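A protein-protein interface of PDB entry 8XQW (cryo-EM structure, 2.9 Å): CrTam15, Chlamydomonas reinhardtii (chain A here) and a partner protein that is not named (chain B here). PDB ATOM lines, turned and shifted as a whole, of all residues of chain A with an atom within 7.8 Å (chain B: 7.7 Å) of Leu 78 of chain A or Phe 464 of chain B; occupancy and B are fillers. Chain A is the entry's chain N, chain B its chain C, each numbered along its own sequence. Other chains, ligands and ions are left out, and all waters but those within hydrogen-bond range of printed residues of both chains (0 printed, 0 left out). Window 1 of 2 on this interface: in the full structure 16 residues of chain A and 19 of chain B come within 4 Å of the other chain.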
ATOM      1  N   ALA A  71      16.153 -24.532 -16.760  1.00  0.00           N
ATOM      2  CA  ALA A  71      16.933 -24.291 -17.966  1.00  0.00           C
ATOM      3  C   ALA A  71      17.741 -23.010 -17.849  1.00  0.00           C
ATOM      4  O   ALA A  71      18.917 -22.974 -18.214  1.00  0.00           O
ATOM      5  CB  ALA A  71      16.016 -24.232 -19.181  1.00  0.00           C
ATOM      6  N   VAL A  72      17.123 -21.941 -17.353  1.00  0.00           N
ATOM      7  CA  VAL A  72      17.866 -20.694 -17.185  1.00  0.00           C
ATOM      8  C   VAL A  72      19.015 -20.884 -16.202  1.00  0.00           C
ATOM      9  O   VAL A  72      20.156 -20.457 -16.451  1.00  0.00           O
ATOM     10  CB  VAL A  72      16.921 -19.568 -16.735  1.00  0.00           C
ATOM     11  CG1 VAL A  72      17.705 -18.320 -16.442  1.00  0.00           C
ATOM     12  CG2 VAL A  72      15.904 -19.294 -17.797  1.00  0.00           C
ATOM     13  N   ALA A  73      18.731 -21.523 -15.068  1.00  0.00           N
ATOM     14  CA  ALA A  73      19.746 -21.648 -14.029  1.00  0.00           C
ATOM     15  C   ALA A  73      20.905 -22.534 -14.456  1.00  0.00           C
ATOM     16  O   ALA A  73      21.993 -22.435 -13.886  1.00  0.00           O
ATOM     17  CB  ALA A  73      19.119 -22.187 -12.752  1.00  0.00           C
ATOM     18  N   ALA A  74      20.694 -23.417 -15.427  1.00  0.00           N
ATOM     19  CA  ALA A  74      21.819 -24.174 -15.967  1.00  0.00           C
ATOM     20  C   ALA A  74      22.505 -23.459 -17.119  1.00  0.00           C
ATOM     21  O   ALA A  74      23.716 -23.624 -17.314  1.00  0.00           O
ATOM     22  CB  ALA A  74      21.356 -25.553 -16.433  1.00  0.00           C
ATOM     23  N   GLY A  75      21.758 -22.669 -17.889  1.00  0.00           N
ATOM     24  CA  GLY A  75      22.368 -21.905 -18.957  1.00  0.00           C
ATOM     25  C   GLY A  75      23.374 -20.899 -18.450  1.00  0.00           C
ATOM     26  O   GLY A  75      24.366 -20.620 -19.122  1.00  0.00           O
ATOM     27  N   TRP A  76      23.139 -20.345 -17.264  1.00  0.00           N
ATOM     28  CA  TRP A  76      24.141 -19.461 -16.672  1.00  0.00           C
ATOM     29  C   TRP A  76      25.492 -20.164 -16.535  1.00  0.00           C
ATOM     30  O   TRP A  76      26.526 -19.663 -17.003  1.00  0.00           O
ATOM     31  CB  TRP A  76      23.653 -18.965 -15.320  1.00  0.00           C
ATOM     32  CG  TRP A  76      24.472 -17.880 -14.765  1.00  0.00           C
ATOM     33  CD1 TRP A  76      24.328 -16.551 -14.998  1.00  0.00           C
ATOM     34  CD2 TRP A  76      25.571 -18.013 -13.865  1.00  0.00           C
ATOM     35  NE1 TRP A  76      25.275 -15.844 -14.307  1.00  0.00           N
ATOM     36  CE2 TRP A  76      26.052 -16.722 -13.601  1.00  0.00           C
ATOM     37  CE3 TRP A  76      26.201 -19.100 -13.260  1.00  0.00           C
ATOM     38  CZ2 TRP A  76      27.128 -16.489 -12.756  1.00  0.00           C
ATOM     39  CZ3 TRP A  76      27.271 -18.865 -12.427  1.00  0.00           C
ATOM     40  CH2 TRP A  76      27.723 -17.573 -12.180  1.00  0.00           C
ATOM     41  N   HIS A  77      25.500 -21.332 -15.894  1.00  0.00           N
ATOM     42  CA  HIS A  77      26.745 -22.067 -15.705  1.00  0.00           C
ATOM     43  C   HIS A  77      27.355 -22.473 -17.035  1.00  0.00           C
ATOM     44  O   HIS A  77      28.581 -22.468 -17.190  1.00  0.00           O
ATOM     45  CB  HIS A  77      26.496 -23.307 -14.852  1.00  0.00           C
ATOM     46  CG  HIS A  77      26.448 -23.039 -13.385  1.00  0.00           C
ATOM     47  ND1 HIS A  77      25.267 -22.927 -12.687  1.00  0.00           N
ATOM     48  CD2 HIS A  77      27.438 -22.890 -12.474  1.00  0.00           C
ATOM     49  CE1 HIS A  77      25.531 -22.708 -11.412  1.00  0.00           C
ATOM     50  NE2 HIS A  77      26.840 -22.678 -11.258  1.00  0.00           N
ATOM     51  N   LEU A  78      26.521 -22.851 -18.003  1.00  0.00           N
ATOM     52  CA  LEU A  78      27.065 -23.259 -19.295  1.00  0.00           C
ATOM     53  C   LEU A  78      27.746 -22.098 -19.999  1.00  0.00           C
ATOM     54  O   LEU A  78      28.784 -22.277 -20.640  1.00  0.00           O
ATOM     55  CB  LEU A  78      25.968 -23.843 -20.175  1.00  0.00           C
ATOM     56  CG  LEU A  78      25.549 -25.255 -19.795  1.00  0.00           C
ATOM     57  CD1 LEU A  78      24.373 -25.688 -20.643  1.00  0.00           C
ATOM     58  CD2 LEU A  78      26.713 -26.216 -19.942  1.00  0.00           C
ATOM     59  N   ALA A  79      27.169 -20.902 -19.903  1.00  0.00           N
ATOM     60  CA  ALA A  79      27.817 -19.731 -20.475  1.00  0.00           C
ATOM     61  C   ALA A  79      29.162 -19.484 -19.818  1.00  0.00           C
ATOM     62  O   ALA A  79      30.155 -19.198 -20.502  1.00  0.00           O
ATOM     63  CB  ALA A  79      26.919 -18.511 -20.331  1.00  0.00           C
ATOM     64  N   SER A  80      29.223 -19.596 -18.494  1.00  0.00           N
ATOM     65  CA  SER A  80      30.508 -19.414 -17.824  1.00  0.00           C
ATOM     66  C   SER A  80      31.534 -20.435 -18.301  1.00  0.00           C
ATOM     67  O   SER A  80      32.705 -20.100 -18.524  1.00  0.00           O
ATOM     68  CB  SER A  80      30.335 -19.505 -16.314  1.00  0.00           C
ATOM     69  OG  SER A  80      31.476 -20.095 -15.726  1.00  0.00           O
ATOM     70  N   PHE A  81      31.111 -21.687 -18.478  1.00  0.00           N
ATOM     71  CA  PHE A  81      32.044 -22.729 -18.900  1.00  0.00           C
ATOM     72  C   PHE A  81      32.513 -22.512 -20.330  1.00  0.00           C
ATOM     73  O   PHE A  81      33.676 -22.766 -20.651  1.00  0.00           O
ATOM     74  CB  PHE A  81      31.396 -24.098 -18.766  1.00  0.00           C
ATOM     75  CG  PHE A  81      32.291 -25.226 -19.156  1.00  0.00           C
ATOM     76  CD1 PHE A  81      33.503 -25.407 -18.527  1.00  0.00           C
ATOM     77  CD2 PHE A  81      31.920 -26.108 -20.144  1.00  0.00           C
ATOM     78  CE1 PHE A  81      34.324 -26.437 -18.882  1.00  0.00           C
ATOM     79  CE2 PHE A  81      32.742 -27.141 -20.501  1.00  0.00           C
ATOM     80  CZ  PHE A  81      33.942 -27.306 -19.869  1.00  0.00           C
ATOM     81  N   ALA A  82      31.627 -22.049 -21.209  1.00  0.00           N
ATOM     82  CA  ALA A  82      32.040 -21.759 -22.576  1.00  0.00           C
ATOM     83  C   ALA A  82      33.038 -20.616 -22.615  1.00  0.00           C
ATOM     84  O   ALA A  82      34.011 -20.652 -23.380  1.00  0.00           O
ATOM     85  CB  ALA A  82      30.827 -21.429 -23.433  1.00  0.00           C
ATOM     86  N   LEU A  83      32.808 -19.583 -21.808  1.00  0.00           N
ATOM     87  CA  LEU A  83      33.785 -18.506 -21.718  1.00  0.00           C
ATOM     88  C   LEU A  83      35.138 -19.026 -21.266  1.00  0.00           C
ATOM     89  O   LEU A  83      36.164 -18.695 -21.859  1.00  0.00           O
ATOM     90  CB  LEU A  83      33.290 -17.435 -20.765  1.00  0.00           C
ATOM     91  CG  LEU A  83      33.827 -16.046 -21.053  1.00  0.00           C
ATOM     92  CD1 LEU A  83      33.136 -15.485 -22.267  1.00  0.00           C
ATOM     93  CD2 LEU A  83      33.598 -15.168 -19.856  1.00  0.00           C
ATOM     94  N   ASN A  84      35.163 -19.843 -20.217  1.00  0.00           N
ATOM     95  CA  ASN A  84      36.435 -20.397 -19.759  1.00  0.00           C
ATOM     96  C   ASN A  84      37.070 -21.280 -20.821  1.00  0.00           C
ATOM     97  O   ASN A  84      38.292 -21.435 -20.857  1.00  0.00           O
ATOM     98  CB  ASN A  84      36.234 -21.183 -18.473  1.00  0.00           C
ATOM     99  CG  ASN A  84      37.485 -21.271 -17.653  1.00  0.00           C
ATOM    100  OD1 ASN A  84      38.563 -20.945 -18.124  1.00  0.00           O
ATOM    101  ND2 ASN A  84      37.353 -21.718 -16.422  1.00  0.00           N
ATOM    102  N   LEU A  85      36.255 -21.893 -21.674  1.00  0.00           N
ATOM    103  CA  LEU A  85      36.797 -22.679 -22.774  1.00  0.00           C
ATOM    104  C   LEU A  85      37.483 -21.802 -23.805  1.00  0.00           C
ATOM    105  O   LEU A  85      38.522 -22.182 -24.348  1.00  0.00           O
ATOM    106  CB  LEU A  85      35.684 -23.466 -23.452  1.00  0.00           C
ATOM    107  CG  LEU A  85      35.520 -24.929 -23.100  1.00  0.00           C
ATOM    108  CD1 LEU A  85      34.553 -25.555 -24.062  1.00  0.00           C
ATOM    109  CD2 LEU A  85      36.853 -25.593 -23.189  1.00  0.00           C
ATOM    110  N   MET B 457      20.546 -21.867  -8.862  1.00  0.00           N
ATOM    111  CA  MET B 457      21.958 -21.766  -9.221  1.00  0.00           C
ATOM    112  C   MET B 457      22.843 -22.356  -8.134  1.00  0.00           C
ATOM    113  O   MET B 457      23.808 -23.074  -8.423  1.00  0.00           O
ATOM    114  CB  MET B 457      22.346 -20.317  -9.471  1.00  0.00           C
ATOM    115  CG  MET B 457      21.846 -19.745 -10.768  1.00  0.00           C
ATOM    116  SD  MET B 457      21.975 -17.954 -10.768  1.00  0.00           S
ATOM    117  CE  MET B 457      21.049 -17.551 -12.235  1.00  0.00           C
ATOM    118  N   ARG B 459      22.021 -24.658  -6.176  1.00  0.00           N
ATOM    119  CA  ARG B 459      21.853 -26.101  -6.245  1.00  0.00           C
ATOM    120  C   ARG B 459      22.779 -26.709  -7.282  1.00  0.00           C
ATOM    121  O   ARG B 459      23.393 -27.750  -7.044  1.00  0.00           O
ATOM    122  CB  ARG B 459      20.404 -26.441  -6.568  1.00  0.00           C
ATOM    123  CG  ARG B 459      20.062 -27.891  -6.401  1.00  0.00           C
ATOM    124  CD  ARG B 459      18.905 -28.049  -5.450  1.00  0.00           C
ATOM    125  NE  ARG B 459      17.705 -27.376  -5.931  1.00  0.00           N
ATOM    126  CZ  ARG B 459      16.833 -26.762  -5.141  1.00  0.00           C
ATOM    127  NH1 ARG B 459      17.032 -26.731  -3.831  1.00  0.00           N
ATOM    128  NH2 ARG B 459      15.763 -26.177  -5.659  1.00  0.00           N
ATOM    129  N   TYR B 460      22.895 -26.068  -8.436  1.00  0.00           N
ATOM    130  CA  TYR B 460      23.685 -26.629  -9.525  1.00  0.00           C
ATOM    131  C   TYR B 460      25.179 -26.402  -9.387  1.00  0.00           C
ATOM    132  O   TYR B 460      25.943 -27.051 -10.100  1.00  0.00           O
ATOM    133  CB  TYR B 460      23.257 -26.041 -10.861  1.00  0.00           C
ATOM    134  CG  TYR B 460      21.991 -26.613 -11.399  1.00  0.00           C
ATOM    135  CD1 TYR B 460      21.571 -27.866 -11.029  1.00  0.00           C
ATOM    136  CD2 TYR B 460      21.213 -25.895 -12.276  1.00  0.00           C
ATOM    137  CE1 TYR B 460      20.414 -28.388 -11.517  1.00  0.00           C
ATOM    138  CE2 TYR B 460      20.058 -26.407 -12.770  1.00  0.00           C
ATOM    139  CZ  TYR B 460      19.661 -27.652 -12.386  1.00  0.00           C
ATOM    140  OH  TYR B 460      18.498 -28.174 -12.881  1.00  0.00           O
ATOM    141  N   THR B 461      25.621 -25.486  -8.527  1.00  0.00           N
ATOM    142  CA  THR B 461      27.018 -25.056  -8.600  1.00  0.00           C
ATOM    143  C   THR B 461      28.026 -26.175  -8.357  1.00  0.00           C
ATOM    144  O   THR B 461      29.175 -26.056  -8.785  1.00  0.00           O
ATOM    145  CB  THR B 461      27.296 -23.934  -7.612  1.00  0.00           C
ATOM    146  OG1 THR B 461      28.692 -23.643  -7.631  1.00  0.00           O
ATOM    147  CG2 THR B 461      26.954 -24.369  -6.235  1.00  0.00           C
ATOM    148  N   VAL B 462      27.657 -27.246  -7.663  1.00  0.00           N
ATOM    149  CA  VAL B 462      28.672 -28.236  -7.290  1.00  0.00           C
ATOM    150  C   VAL B 462      29.007 -29.196  -8.431  1.00  0.00           C
ATOM    151  O   VAL B 462      30.198 -29.379  -8.735  1.00  0.00           O
ATOM    152  CB  VAL B 462      28.260 -29.013  -6.033  1.00  0.00           C
ATOM    153  CG1 VAL B 462      29.131 -30.235  -5.875  1.00  0.00           C
ATOM    154  CG2 VAL B 462      28.374 -28.133  -4.814  1.00  0.00           C
ATOM    155  N   PRO B 463      28.031 -29.836  -9.087  1.00  0.00           N
ATOM    156  CA  PRO B 463      28.395 -30.720 -10.205  1.00  0.00           C
ATOM    157  C   PRO B 463      29.125 -30.009 -11.327  1.00  0.00           C
ATOM    158  O   PRO B 463      30.078 -30.559 -11.893  1.00  0.00           O
ATOM    159  CB  PRO B 463      27.040 -31.263 -10.670  1.00  0.00           C
ATOM    160  CG  PRO B 463      26.047 -30.328 -10.128  1.00  0.00           C
ATOM    161  CD  PRO B 463      26.590 -29.909  -8.820  1.00  0.00           C
ATOM    162  N   PHE B 464      28.691 -28.802 -11.680  1.00  0.00           N
ATOM    163  CA  PHE B 464      29.419 -28.041 -12.684  1.00  0.00           C
ATOM    164  C   PHE B 464      30.844 -27.781 -12.235  1.00  0.00           C
ATOM    165  O   PHE B 464      31.777 -27.850 -13.040  1.00  0.00           O
ATOM    166  CB  PHE B 464      28.699 -26.736 -12.970  1.00  0.00           C
ATOM    167  CG  PHE B 464      27.621 -26.863 -13.991  1.00  0.00           C
ATOM    168  CD1 PHE B 464      26.332 -27.176 -13.621  1.00  0.00           C
ATOM    169  CD2 PHE B 464      27.894 -26.670 -15.326  1.00  0.00           C
ATOM    170  CE1 PHE B 464      25.339 -27.287 -14.558  1.00  0.00           C
ATOM    171  CE2 PHE B 464      26.904 -26.785 -16.264  1.00  0.00           C
ATOM    172  CZ  PHE B 464      25.625 -27.093 -15.876  1.00  0.00           C
ATOM    173  N   MET B 465      31.035 -27.511 -10.948  1.00  0.00           N
ATOM    174  CA  MET B 465      32.380 -27.278 -10.443  1.00  0.00           C
ATOM    175  C   MET B 465      33.248 -28.512 -10.604  1.00  0.00           C
ATOM    176  O   MET B 465      34.411 -28.410 -11.008  1.00  0.00           O
ATOM    177  CB  MET B 465      32.326 -26.840  -8.983  1.00  0.00           C
ATOM    178  CG  MET B 465      33.557 -26.091  -8.511  1.00  0.00           C
ATOM    179  SD  MET B 465      33.886 -24.594  -9.459  1.00  0.00           S
ATOM    180  CE  MET B 465      32.287 -23.800  -9.420  1.00  0.00           C
ATOM    181  N   VAL B 466      32.702 -29.696 -10.329  1.00  0.00           N
ATOM    182  CA  VAL B 466      33.540 -30.890 -10.406  1.00  0.00           C
ATOM    183  C   VAL B 466      33.833 -31.256 -11.857  1.00  0.00           C
ATOM    184  O   VAL B 466      34.925 -31.734 -12.177  1.00  0.00           O
ATOM    185  CB  VAL B 466      32.922 -32.065  -9.629  1.00  0.00           C
ATOM    186  CG1 VAL B 466      32.444 -31.603  -8.275  1.00  0.00           C
ATOM    187  CG2 VAL B 466      31.807 -32.722 -10.407  1.00  0.00           C
ATOM    188  N   ILE B 467      32.886 -31.026 -12.769  1.00  0.00           N
ATOM    189  CA  ILE B 467      33.197 -31.378 -14.151  1.00  0.00           C
ATOM    190  C   ILE B 467      34.178 -30.379 -14.742  1.00  0.00           C
ATOM    191  O   ILE B 467      35.029 -30.741 -15.562  1.00  0.00           O
ATOM    192  CB  ILE B 467      31.939 -31.512 -15.024  1.00  0.00           C
ATOM    193  CG1 ILE B 467      31.279 -30.160 -15.259  1.00  0.00           C
ATOM    194  CG2 ILE B 467      30.982 -32.501 -14.415  1.00  0.00           C
ATOM    195  CD1 ILE B 467      31.006 -29.878 -16.720  1.00  0.00           C
ATOM    196  N   SER B 468      34.114 -29.119 -14.312  1.00  0.00           N
ATOM    197  CA  SER B 468      35.130 -28.169 -14.746  1.00  0.00           C
ATOM    198  C   SER B 468      36.501 -28.554 -14.206  1.00  0.00           C
ATOM    199  O   SER B 468      37.498 -28.509 -14.935  1.00  0.00           O
ATOM    200  CB  SER B 468      34.748 -26.761 -14.303  1.00  0.00           C
ATOM    201  OG  SER B 468      35.431 -25.782 -15.061  1.00  0.00           O
ATOM    202  N   GLY B 469      36.567 -28.957 -12.938  1.00  0.00           N
ATOM    203  CA  GLY B 469      37.834 -29.396 -12.382  1.00  0.00           C
ATOM    204  C   GLY B 469      38.416 -30.587 -13.115  1.00  0.00           C
ATOM    205  O   GLY B 469      39.610 -30.613 -13.426  1.00  0.00           O
ATOM    206  N   LEU B 470      37.585 -31.584 -13.417  1.00  0.00           N
ATOM    207  CA  LEU B 470      38.078 -32.743 -14.154  1.00  0.00           C
ATOM    208  C   LEU B 470      38.561 -32.350 -15.539  1.00  0.00           C
ATOM    209  O   LEU B 470      39.632 -32.789 -15.981  1.00  0.00           O
ATOM    210  CB  LEU B 470      36.991 -33.804 -14.261  1.00  0.00           C
ATOM    211  CG  LEU B 470      36.653 -34.574 -12.991  1.00  0.00           C
ATOM    212  CD1 LEU B 470      35.813 -35.782 -13.333  1.00  0.00           C
ATOM    213  CD2 LEU B 470      37.913 -34.987 -12.263  1.00  0.00           C
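Trp 76 of chain A touches none of the printed residues of chain B. Of the printed residues of chain B, His 77 of chain A touches Met 457 (3.5 Å), Thr 461 (3.6 Å) and Phe 464 (3.7 Å). Leu 78 of chain A touches just one residue of chain B: Phe 464. Printed residues of chain A within 4 Å of Thr 461 of chain B: His 77. No residue of chain A comes within 4 Å of Pro 463 of chain B. The nearest residue of chain A that does not touch Phe 464 of chain B is Ala 74 of chain A (4.2 Å). The nearest printed residue of chain A that does not touch Met 457 of chain B is Ala 73 of chain A (4.1 Å).
Of the 15 printed residues of chain A, 5 touch a printed residue of chain B. Along chain A the printed residues that touch a printed residue of chain B span positions 73 to 81. Hydrophobic or aromatic side chains of chain B within 4 Å of the printed part of chain A: Tyr 460 and Phe 464. Among the printed residues, no Asp or Glu carboxylate lies within 4 Å of a Lys or Arg side-chain nitrogen of the other chain.
Among the printed residues, pairs that only touch across the chains: His 77 of chain A with Met 457 of chain B (3.5 Å), His 77 of chain A with Thr 461 of chain B (3.6 Å), His 77 of chain A with Phe 464 of chain B (3.7 Å), Leu 78 of chain A with Phe 464 of chain B (3.7 Å), Ala 73 of chain A with Tyr 460 of chain B (3.9 Å), Ala 74 of chain A with Tyr 460 of chain B (3.98 Å) and Phe 81 of chain A with Ser 468 of chain B (3.98 Å).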
